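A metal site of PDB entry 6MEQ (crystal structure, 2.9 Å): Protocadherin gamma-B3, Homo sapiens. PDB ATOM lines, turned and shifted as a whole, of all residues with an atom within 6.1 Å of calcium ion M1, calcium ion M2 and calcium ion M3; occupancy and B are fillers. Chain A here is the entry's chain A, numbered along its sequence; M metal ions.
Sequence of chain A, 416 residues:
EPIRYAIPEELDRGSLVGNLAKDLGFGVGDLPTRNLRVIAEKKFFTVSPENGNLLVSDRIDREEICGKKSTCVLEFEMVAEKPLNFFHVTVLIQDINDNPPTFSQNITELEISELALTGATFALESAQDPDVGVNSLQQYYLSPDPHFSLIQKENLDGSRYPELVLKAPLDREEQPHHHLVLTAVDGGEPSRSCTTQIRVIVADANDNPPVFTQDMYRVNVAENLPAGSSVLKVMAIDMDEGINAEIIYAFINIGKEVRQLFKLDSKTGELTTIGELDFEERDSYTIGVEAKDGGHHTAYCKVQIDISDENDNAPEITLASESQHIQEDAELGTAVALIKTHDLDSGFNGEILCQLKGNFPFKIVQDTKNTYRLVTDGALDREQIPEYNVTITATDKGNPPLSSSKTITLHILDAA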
ATOM      1  N   GLU A   9      10.316 -19.085  -9.003  1.00  0.00           N
ATOM      2  CA  GLU A   9      10.831 -19.465  -7.696  1.00  0.00           C
ATOM      3  C   GLU A   9      11.168 -18.228  -6.875  1.00  0.00           C
ATOM      4  O   GLU A   9      11.153 -17.085  -7.369  1.00  0.00           O
ATOM      5  CB  GLU A   9      12.055 -20.357  -7.842  1.00  0.00           C
ATOM      6  CG  GLU A   9      13.190 -19.720  -8.645  1.00  0.00           C
ATOM      7  CD  GLU A   9      14.500 -20.452  -8.485  1.00  0.00           C
ATOM      8  OE1 GLU A   9      14.666 -21.155  -7.466  1.00  0.00           O
ATOM      9  OE2 GLU A   9      15.366 -20.324  -9.377  1.00  0.00           O
ATOM     10  N   GLU A  10      11.482 -18.462  -5.600  1.00  0.00           N
ATOM     11  CA  GLU A  10      11.918 -17.414  -4.673  1.00  0.00           C
ATOM     12  C   GLU A  10      10.860 -16.319  -4.530  1.00  0.00           C
ATOM     13  O   GLU A  10      11.174 -15.133  -4.404  1.00  0.00           O
ATOM     14  CB  GLU A  10      13.255 -16.817  -5.093  1.00  0.00           C
ATOM     15  CG  GLU A  10      14.384 -17.840  -5.229  1.00  0.00           C
ATOM     16  CD  GLU A  10      14.785 -18.443  -3.895  1.00  0.00           C
ATOM     17  OE1 GLU A  10      14.482 -17.844  -2.846  1.00  0.00           O
ATOM     18  OE2 GLU A  10      15.408 -19.521  -3.906  1.00  0.00           O
ATOM     19  N   ARG A  59       9.797 -20.905   1.503  1.00  0.00           N
ATOM     20  CA  ARG A  59      10.703 -20.561   0.417  1.00  0.00           C
ATOM     21  C   ARG A  59      10.837 -21.724  -0.547  1.00  0.00           C
ATOM     22  O   ARG A  59      11.110 -22.859  -0.145  1.00  0.00           O
ATOM     23  CB  ARG A  59      12.076 -20.173   0.978  1.00  0.00           C
ATOM     24  CG  ARG A  59      13.122 -19.897  -0.079  1.00  0.00           C
ATOM     25  CD  ARG A  59      14.430 -19.425   0.549  1.00  0.00           C
ATOM     26  NE  ARG A  59      15.487 -19.246  -0.446  1.00  0.00           N
ATOM     27  CZ  ARG A  59      16.378 -20.176  -0.764  1.00  0.00           C
ATOM     28  NH1 ARG A  59      16.353 -21.353  -0.165  1.00  0.00           N
ATOM     29  NH2 ARG A  59      17.307 -19.915  -1.679  1.00  0.00           N
ATOM     30  N   ILE A  60      10.645 -21.445  -1.836  1.00  0.00           N
ATOM     31  CA  ILE A  60      10.705 -22.457  -2.881  1.00  0.00           C
ATOM     32  C   ILE A  60      12.009 -22.228  -3.648  1.00  0.00           C
ATOM     33  O   ILE A  60      12.086 -21.356  -4.517  1.00  0.00           O
ATOM     34  CB  ILE A  60       9.485 -22.396  -3.814  1.00  0.00           C
ATOM     35  CG1 ILE A  60       8.202 -22.569  -3.011  1.00  0.00           C
ATOM     36  CG2 ILE A  60       9.589 -23.465  -4.900  1.00  0.00           C
ATOM     37  CD1 ILE A  60       6.943 -22.515  -3.850  1.00  0.00           C
ATOM     38  N   ASP A  61      13.030 -23.007  -3.316  1.00  0.00           N
ATOM     39  CA  ASP A  61      14.327 -22.931  -3.971  1.00  0.00           C
ATOM     40  C   ASP A  61      14.417 -24.063  -4.989  1.00  0.00           C
ATOM     41  O   ASP A  61      14.486 -25.234  -4.616  1.00  0.00           O
ATOM     42  CB  ASP A  61      15.465 -23.015  -2.951  1.00  0.00           C
ATOM     43  CG  ASP A  61      16.826 -22.776  -3.565  1.00  0.00           C
ATOM     44  OD1 ASP A  61      16.894 -22.350  -4.747  1.00  0.00           O
ATOM     45  OD2 ASP A  61      17.841 -23.012  -2.882  1.00  0.00           O
ATOM     46  N   ARG A  62      14.418 -23.709  -6.277  1.00  0.00           N
ATOM     47  CA  ARG A  62      14.444 -24.733  -7.318  1.00  0.00           C
ATOM     48  C   ARG A  62      15.746 -25.514  -7.315  1.00  0.00           C
ATOM     49  O   ARG A  62      15.759 -26.704  -7.672  1.00  0.00           O
ATOM     50  CB  ARG A  62      14.219 -24.087  -8.691  1.00  0.00           C
ATOM     51  CG  ARG A  62      13.923 -25.082  -9.796  1.00  0.00           C
ATOM     52  CD  ARG A  62      14.368 -24.566 -11.146  1.00  0.00           C
ATOM     53  NE  ARG A  62      15.801 -24.313 -11.177  1.00  0.00           N
ATOM     54  CZ  ARG A  62      16.716 -25.249 -11.415  1.00  0.00           C
ATOM     55  NH1 ARG A  62      16.338 -26.496 -11.655  1.00  0.00           N
ATOM     56  NH2 ARG A  62      18.006 -24.933 -11.423  1.00  0.00           N
ATOM     57  N   GLU A  63      16.855 -24.884  -6.920  1.00  0.00           N
ATOM     58  CA  GLU A  63      18.130 -25.595  -6.886  1.00  0.00           C
ATOM     59  C   GLU A  63      18.167 -26.635  -5.778  1.00  0.00           C
ATOM     60  O   GLU A  63      18.887 -27.634  -5.904  1.00  0.00           O
ATOM     61  CB  GLU A  63      19.286 -24.591  -6.722  1.00  0.00           C
ATOM     62  CG  GLU A  63      19.655 -23.840  -7.985  1.00  0.00           C
ATOM     63  CD  GLU A  63      18.590 -22.854  -8.420  1.00  0.00           C
ATOM     64  OE1 GLU A  63      17.998 -22.187  -7.538  1.00  0.00           O
ATOM     65  OE2 GLU A  63      18.341 -22.746  -9.646  1.00  0.00           O
ATOM     66  N   ASP A  95      12.507 -21.256 -13.314  1.00  0.00           N
ATOM     67  CA  ASP A  95      13.861 -20.968 -12.858  1.00  0.00           C
ATOM     68  C   ASP A  95      14.225 -19.517 -13.141  1.00  0.00           C
ATOM     69  O   ASP A  95      13.963 -18.999 -14.233  1.00  0.00           O
ATOM     70  CB  ASP A  95      14.867 -21.905 -13.530  1.00  0.00           C
ATOM     71  CG  ASP A  95      16.296 -21.578 -13.144  1.00  0.00           C
ATOM     72  OD1 ASP A  95      16.647 -21.738 -11.960  1.00  0.00           O
ATOM     73  OD2 ASP A  95      17.070 -21.165 -14.034  1.00  0.00           O
ATOM     74  N   ILE A  96      14.834 -18.869 -12.154  1.00  0.00           N
ATOM     75  CA  ILE A  96      15.334 -17.512 -12.296  1.00  0.00           C
ATOM     76  C   ILE A  96      16.851 -17.539 -12.140  1.00  0.00           C
ATOM     77  O   ILE A  96      17.420 -18.452 -11.538  1.00  0.00           O
ATOM     78  CB  ILE A  96      14.701 -16.542 -11.279  1.00  0.00           C
ATOM     79  CG1 ILE A  96      15.126 -16.903  -9.857  1.00  0.00           C
ATOM     80  CG2 ILE A  96      13.191 -16.537 -11.412  1.00  0.00           C
ATOM     81  CD1 ILE A  96      14.572 -15.967  -8.795  1.00  0.00           C
ATOM     82  N   ASN A  97      17.503 -16.521 -12.706  1.00  0.00           N
ATOM     83  CA  ASN A  97      18.957 -16.415 -12.662  1.00  0.00           C
ATOM     84  C   ASN A  97      19.347 -15.709 -11.364  1.00  0.00           C
ATOM     85  O   ASN A  97      19.629 -14.510 -11.323  1.00  0.00           O
ATOM     86  CB  ASN A  97      19.490 -15.688 -13.885  1.00  0.00           C
ATOM     87  CG  ASN A  97      20.998 -15.678 -13.941  1.00  0.00           C
ATOM     88  OD1 ASN A  97      21.656 -16.530 -13.362  1.00  0.00           O
ATOM     89  ND2 ASN A  97      21.562 -14.697 -14.651  1.00  0.00           N
ATOM     90  N   ASP A  98      19.369 -16.484 -10.280  1.00  0.00           N
ATOM     91  CA  ASP A  98      19.719 -15.969  -8.962  1.00  0.00           C
ATOM     92  C   ASP A  98      20.982 -16.615  -8.403  1.00  0.00           C
ATOM     93  O   ASP A  98      21.259 -16.507  -7.207  1.00  0.00           O
ATOM     94  CB  ASP A  98      18.550 -16.159  -7.986  1.00  0.00           C
ATOM     95  CG  ASP A  98      18.078 -17.596  -7.911  1.00  0.00           C
ATOM     96  OD1 ASP A  98      18.553 -18.426  -8.700  1.00  0.00           O
ATOM     97  OD2 ASP A  98      17.224 -17.886  -7.045  1.00  0.00           O
ATOM     98  N   ASN A  99      21.763 -17.286  -9.256  1.00  0.00           N
ATOM     99  CA  ASN A  99      22.989 -17.936  -8.820  1.00  0.00           C
ATOM    100  C   ASN A  99      24.106 -17.686  -9.827  1.00  0.00           C
ATOM    101  O   ASN A  99      23.978 -18.080 -10.995  1.00  0.00           O
ATOM    102  CB  ASN A  99      22.766 -19.439  -8.632  1.00  0.00           C
ATOM    103  CG  ASN A  99      21.875 -19.746  -7.438  1.00  0.00           C
ATOM    104  OD1 ASN A  99      20.785 -20.296  -7.592  1.00  0.00           O
ATOM    105  ND2 ASN A  99      22.343 -19.404  -6.241  1.00  0.00           N
ATOM    106  N   PRO A 100      25.196 -17.055  -9.418  1.00  0.00           N
ATOM    107  CA  PRO A 100      26.296 -16.789 -10.350  1.00  0.00           C
ATOM    108  C   PRO A 100      27.117 -18.038 -10.597  1.00  0.00           C
ATOM    109  O   PRO A 100      27.129 -18.953  -9.754  1.00  0.00           O
ATOM    110  CB  PRO A 100      27.114 -15.717  -9.615  1.00  0.00           C
ATOM    111  CG  PRO A 100      26.876 -15.999  -8.180  1.00  0.00           C
ATOM    112  CD  PRO A 100      25.454 -16.493  -8.083  1.00  0.00           C
ATOM    113  N   PRO A 101      27.793 -18.123 -11.733  1.00  0.00           N
ATOM    114  CA  PRO A 101      28.687 -19.264 -11.972  1.00  0.00           C
ATOM    115  C   PRO A 101      29.916 -19.185 -11.069  1.00  0.00           C
ATOM    116  O   PRO A 101      30.194 -18.173 -10.431  1.00  0.00           O
ATOM    117  CB  PRO A 101      29.062 -19.116 -13.442  1.00  0.00           C
ATOM    118  CG  PRO A 101      28.902 -17.660 -13.728  1.00  0.00           C
ATOM    119  CD  PRO A 101      27.752 -17.205 -12.882  1.00  0.00           C
ATOM    120  N   ASP A 129      27.253 -23.914 -12.833  1.00  0.00           N
ATOM    121  CA  ASP A 129      26.163 -23.057 -12.395  1.00  0.00           C
ATOM    122  C   ASP A 129      24.996 -23.919 -11.934  1.00  0.00           C
ATOM    123  O   ASP A 129      24.511 -24.768 -12.694  1.00  0.00           O
ATOM    124  CB  ASP A 129      25.737 -22.134 -13.537  1.00  0.00           C
ATOM    125  CG  ASP A 129      24.926 -20.941 -13.051  1.00  0.00           C
ATOM    126  OD1 ASP A 129      24.012 -21.124 -12.222  1.00  0.00           O
ATOM    127  OD2 ASP A 129      25.202 -19.810 -13.510  1.00  0.00           O
ATOM    128  N   PRO A 130      24.522 -23.742 -10.695  1.00  0.00           N
ATOM    129  CA  PRO A 130      23.405 -24.570 -10.212  1.00  0.00           C
ATOM    130  C   PRO A 130      22.081 -24.298 -10.917  1.00  0.00           C
ATOM    131  O   PRO A 130      21.132 -25.055 -10.721  1.00  0.00           O
ATOM    132  CB  PRO A 130      23.321 -24.205  -8.722  1.00  0.00           C
ATOM    133  CG  PRO A 130      23.932 -22.854  -8.633  1.00  0.00           C
ATOM    134  CD  PRO A 130      25.025 -22.817  -9.664  1.00  0.00           C
ATOM    135  N   ASP A 131      21.990 -23.243 -11.726  1.00  0.00           N
ATOM    136  CA  ASP A 131      20.772 -22.949 -12.470  1.00  0.00           C
ATOM    137  C   ASP A 131      20.656 -23.896 -13.667  1.00  0.00           C
ATOM    138  O   ASP A 131      21.512 -24.742 -13.915  1.00  0.00           O
ATOM    139  CB  ASP A 131      20.757 -21.487 -12.907  1.00  0.00           C
ATOM    140  CG  ASP A 131      20.793 -20.520 -11.738  1.00  0.00           C
ATOM    141  OD1 ASP A 131      20.230 -20.858 -10.677  1.00  0.00           O
ATOM    142  OD2 ASP A 131      21.383 -19.432 -11.886  1.00  0.00           O
ATOM    143  N   VAL A 132      19.567 -23.748 -14.417  1.00  0.00           N
ATOM    144  CA  VAL A 132      19.307 -24.552 -15.606  1.00  0.00           C
ATOM    145  C   VAL A 132      18.890 -23.624 -16.738  1.00  0.00           C
ATOM    146  O   VAL A 132      18.649 -22.432 -16.541  1.00  0.00           O
ATOM    147  CB  VAL A 132      18.233 -25.630 -15.360  1.00  0.00           C
ATOM    148  CG1 VAL A 132      18.703 -26.640 -14.324  1.00  0.00           C
ATOM    149  CG2 VAL A 132      16.916 -24.988 -14.942  1.00  0.00           C
ATOM    150  N   ASN A 135      19.994 -19.718 -17.994  1.00  0.00           N
ATOM    151  CA  ASN A 135      20.606 -19.157 -16.788  1.00  0.00           C
ATOM    152  C   ASN A 135      21.915 -19.837 -16.437  1.00  0.00           C
ATOM    153  O   ASN A 135      22.709 -19.270 -15.685  1.00  0.00           O
ATOM    154  CB  ASN A 135      19.637 -19.252 -15.611  1.00  0.00           C
ATOM    155  CG  ASN A 135      18.313 -18.558 -15.878  1.00  0.00           C
ATOM    156  OD1 ASN A 135      18.258 -17.593 -16.639  1.00  0.00           O
ATOM    157  ND2 ASN A 135      17.252 -19.047 -15.259  1.00  0.00           N
ATOM    158  N   SER A 136      22.171 -21.032 -16.974  1.00  0.00           N
ATOM    159  CA  SER A 136      23.422 -21.736 -16.758  1.00  0.00           C
ATOM    160  C   SER A 136      24.299 -21.802 -18.011  1.00  0.00           C
ATOM    161  O   SER A 136      25.432 -22.272 -17.925  1.00  0.00           O
ATOM    162  CB  SER A 136      23.159 -23.159 -16.262  1.00  0.00           C
ATOM    163  OG  SER A 136      22.413 -23.908 -17.207  1.00  0.00           O
ATOM    164  N   GLN A 138      26.917 -20.767 -20.152  1.00  0.00           N
ATOM    165  CA  GLN A 138      28.044 -19.883 -19.891  1.00  0.00           C
ATOM    166  C   GLN A 138      28.659 -19.382 -21.201  1.00  0.00           C
ATOM    167  O   GLN A 138      28.612 -20.046 -22.231  1.00  0.00           O
ATOM    168  CB  GLN A 138      29.113 -20.601 -19.072  1.00  0.00           C
ATOM    169  CG  GLN A 138      28.602 -21.151 -17.750  1.00  0.00           C
ATOM    170  CD  GLN A 138      28.050 -20.077 -16.836  1.00  0.00           C
ATOM    171  OE1 GLN A 138      28.521 -18.938 -16.840  1.00  0.00           O
ATOM    172  NE2 GLN A 138      27.046 -20.442 -16.048  1.00  0.00           N
ATOM    173  N   ASP A 186      27.023 -15.943 -17.728  1.00  0.00           N
ATOM    174  CA  ASP A 186      25.864 -16.746 -18.094  1.00  0.00           C
ATOM    175  C   ASP A 186      24.903 -15.928 -18.958  1.00  0.00           C
ATOM    176  O   ASP A 186      25.030 -14.705 -19.100  1.00  0.00           O
ATOM    177  CB  ASP A 186      25.154 -17.277 -16.847  1.00  0.00           C
ATOM    178  CG  ASP A 186      24.705 -16.175 -15.905  1.00  0.00           C
ATOM    179  OD1 ASP A 186      24.929 -14.983 -16.211  1.00  0.00           O
ATOM    180  OD2 ASP A 186      24.119 -16.507 -14.847  1.00  0.00           O
ATOM    181  N   ARG A 192      25.126 -12.611 -14.370  1.00  0.00           N
ATOM    182  CA  ARG A 192      26.088 -12.819 -13.296  1.00  0.00           C
ATOM    183  C   ARG A 192      27.337 -13.476 -13.855  1.00  0.00           C
ATOM    184  O   ARG A 192      27.257 -14.328 -14.746  1.00  0.00           O
ATOM    185  CB  ARG A 192      25.486 -13.669 -12.185  1.00  0.00           C
ATOM    186  CG  ARG A 192      24.473 -12.924 -11.316  1.00  0.00           C
ATOM    187  CD  ARG A 192      23.871 -13.844 -10.262  1.00  0.00           C
ATOM    188  NE  ARG A 192      23.133 -13.102  -9.244  1.00  0.00           N
ATOM    189  CZ  ARG A 192      21.874 -12.717  -9.372  1.00  0.00           C
ATOM    190  NH1 ARG A 192      21.196 -13.003 -10.478  1.00  0.00           N
ATOM    191  NH2 ARG A 192      21.278 -12.049  -8.392  1.00  0.00           N
HETATM  192 CA    CA M   1      17.086 -20.292  -6.158  1.00  0.00          CA
HETATM  193 CA    CA M   2      17.764 -20.429 -10.044  1.00  0.00          CA
HETATM  194 CA    CA M   3      23.108 -18.536 -13.360  1.00  0.00          CA
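The side-chain amide oxygen (OE1) of Gln 138 sits at hydrogen-bond distance from the backbone NH (N) of Asp 186 (3.5 Å). The guanidinium group of Arg 59 lies within salt-bridge range of the side-chain carboxylate of Glu 10 (3.0 Å). N of Arg 192 sits at hydrogen-bond distance from OD1 of Asp 186 (3.0 Å). The side-chain carboxylate (OD2) of Asp 61 is in salt-bridge range of the guanidinium group (NH2) of Arg 59 (3.4 Å). The side-chain carboxylate (OD2) of Asp 129 lies close to the side-chain amide nitrogen (NE2) of Gln 138 (3.2 Å). The side-chain carboxylate of Glu 63 sits close to the guanidinium group of Arg 62 (2.8 Å). OD1 of Asp 95 lies close to NE of Arg 62, 2.8 Å away. N of Arg 62 lies close to OE1 of Glu 9, at 2.8 Å.
Of the 23 residues printed, 6 come within 4 Å of calcium ion M1.
The nearest printed residue that does not touch calcium ion M2 is Arg 62 (4.5 Å).
Six residues have an atom within 4 Å of calcium ion M3: Asn 97, Asn 99, Asp 129, Asp 131, Asn 135 and Asp 186. The nearest printed residue that does not touch calcium ion M3 is Ser 136 (4.5 Å).
Calcium ion M1 is bound by the side-chain carboxylate of Asp 61, the side-chain carboxylate of Glu 63, the side-chain carboxylate of Asp 98 and the side-chain carboxylate of Glu 9. Slightly farther from calcium ion M1 lies OE2 of Glu 10 (2.9 Å).
Calcium ion M2 is bound by the side-chain carboxylate (OE2) of Glu 63, the side-chain carboxylate (OE2) of Glu 9, the backbone carbonyl oxygen (O) of Ile 96, the side-chain carboxylate (OD1) of Asp 98, the side-chain carboxylate (OD1) of Asp 95 and the side-chain carboxylate (OD1) of Asp 131. Calcium ion M2 has six donor atoms within binding distance. Slightly farther from calcium ion M2 lies the side-chain carboxylate (OE1) of Glu 63 (3.1 Å).
OD2 of Asp 131 binds calcium ion M3, at 2.4 Å. The side-chain carboxylate (OD2) of Asp 129 binds calcium ion M3 (2.5 Å). O of Asn 135 is bound to calcium ion M3. The side-chain amide oxygen (OD1) of Asn 97 is bound to calcium ion M3 (2.5 Å). Calcium ion M3 is bound by O of Asn 99, 2.6 Å away. OD2 of Asp 186 is bound to calcium ion M3, at 2.7 Å. Calcium ion M3 has six donor atoms within binding distance. Slightly farther from calcium ion M3 lies OD1 of Asp 129 (3.0 Å).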
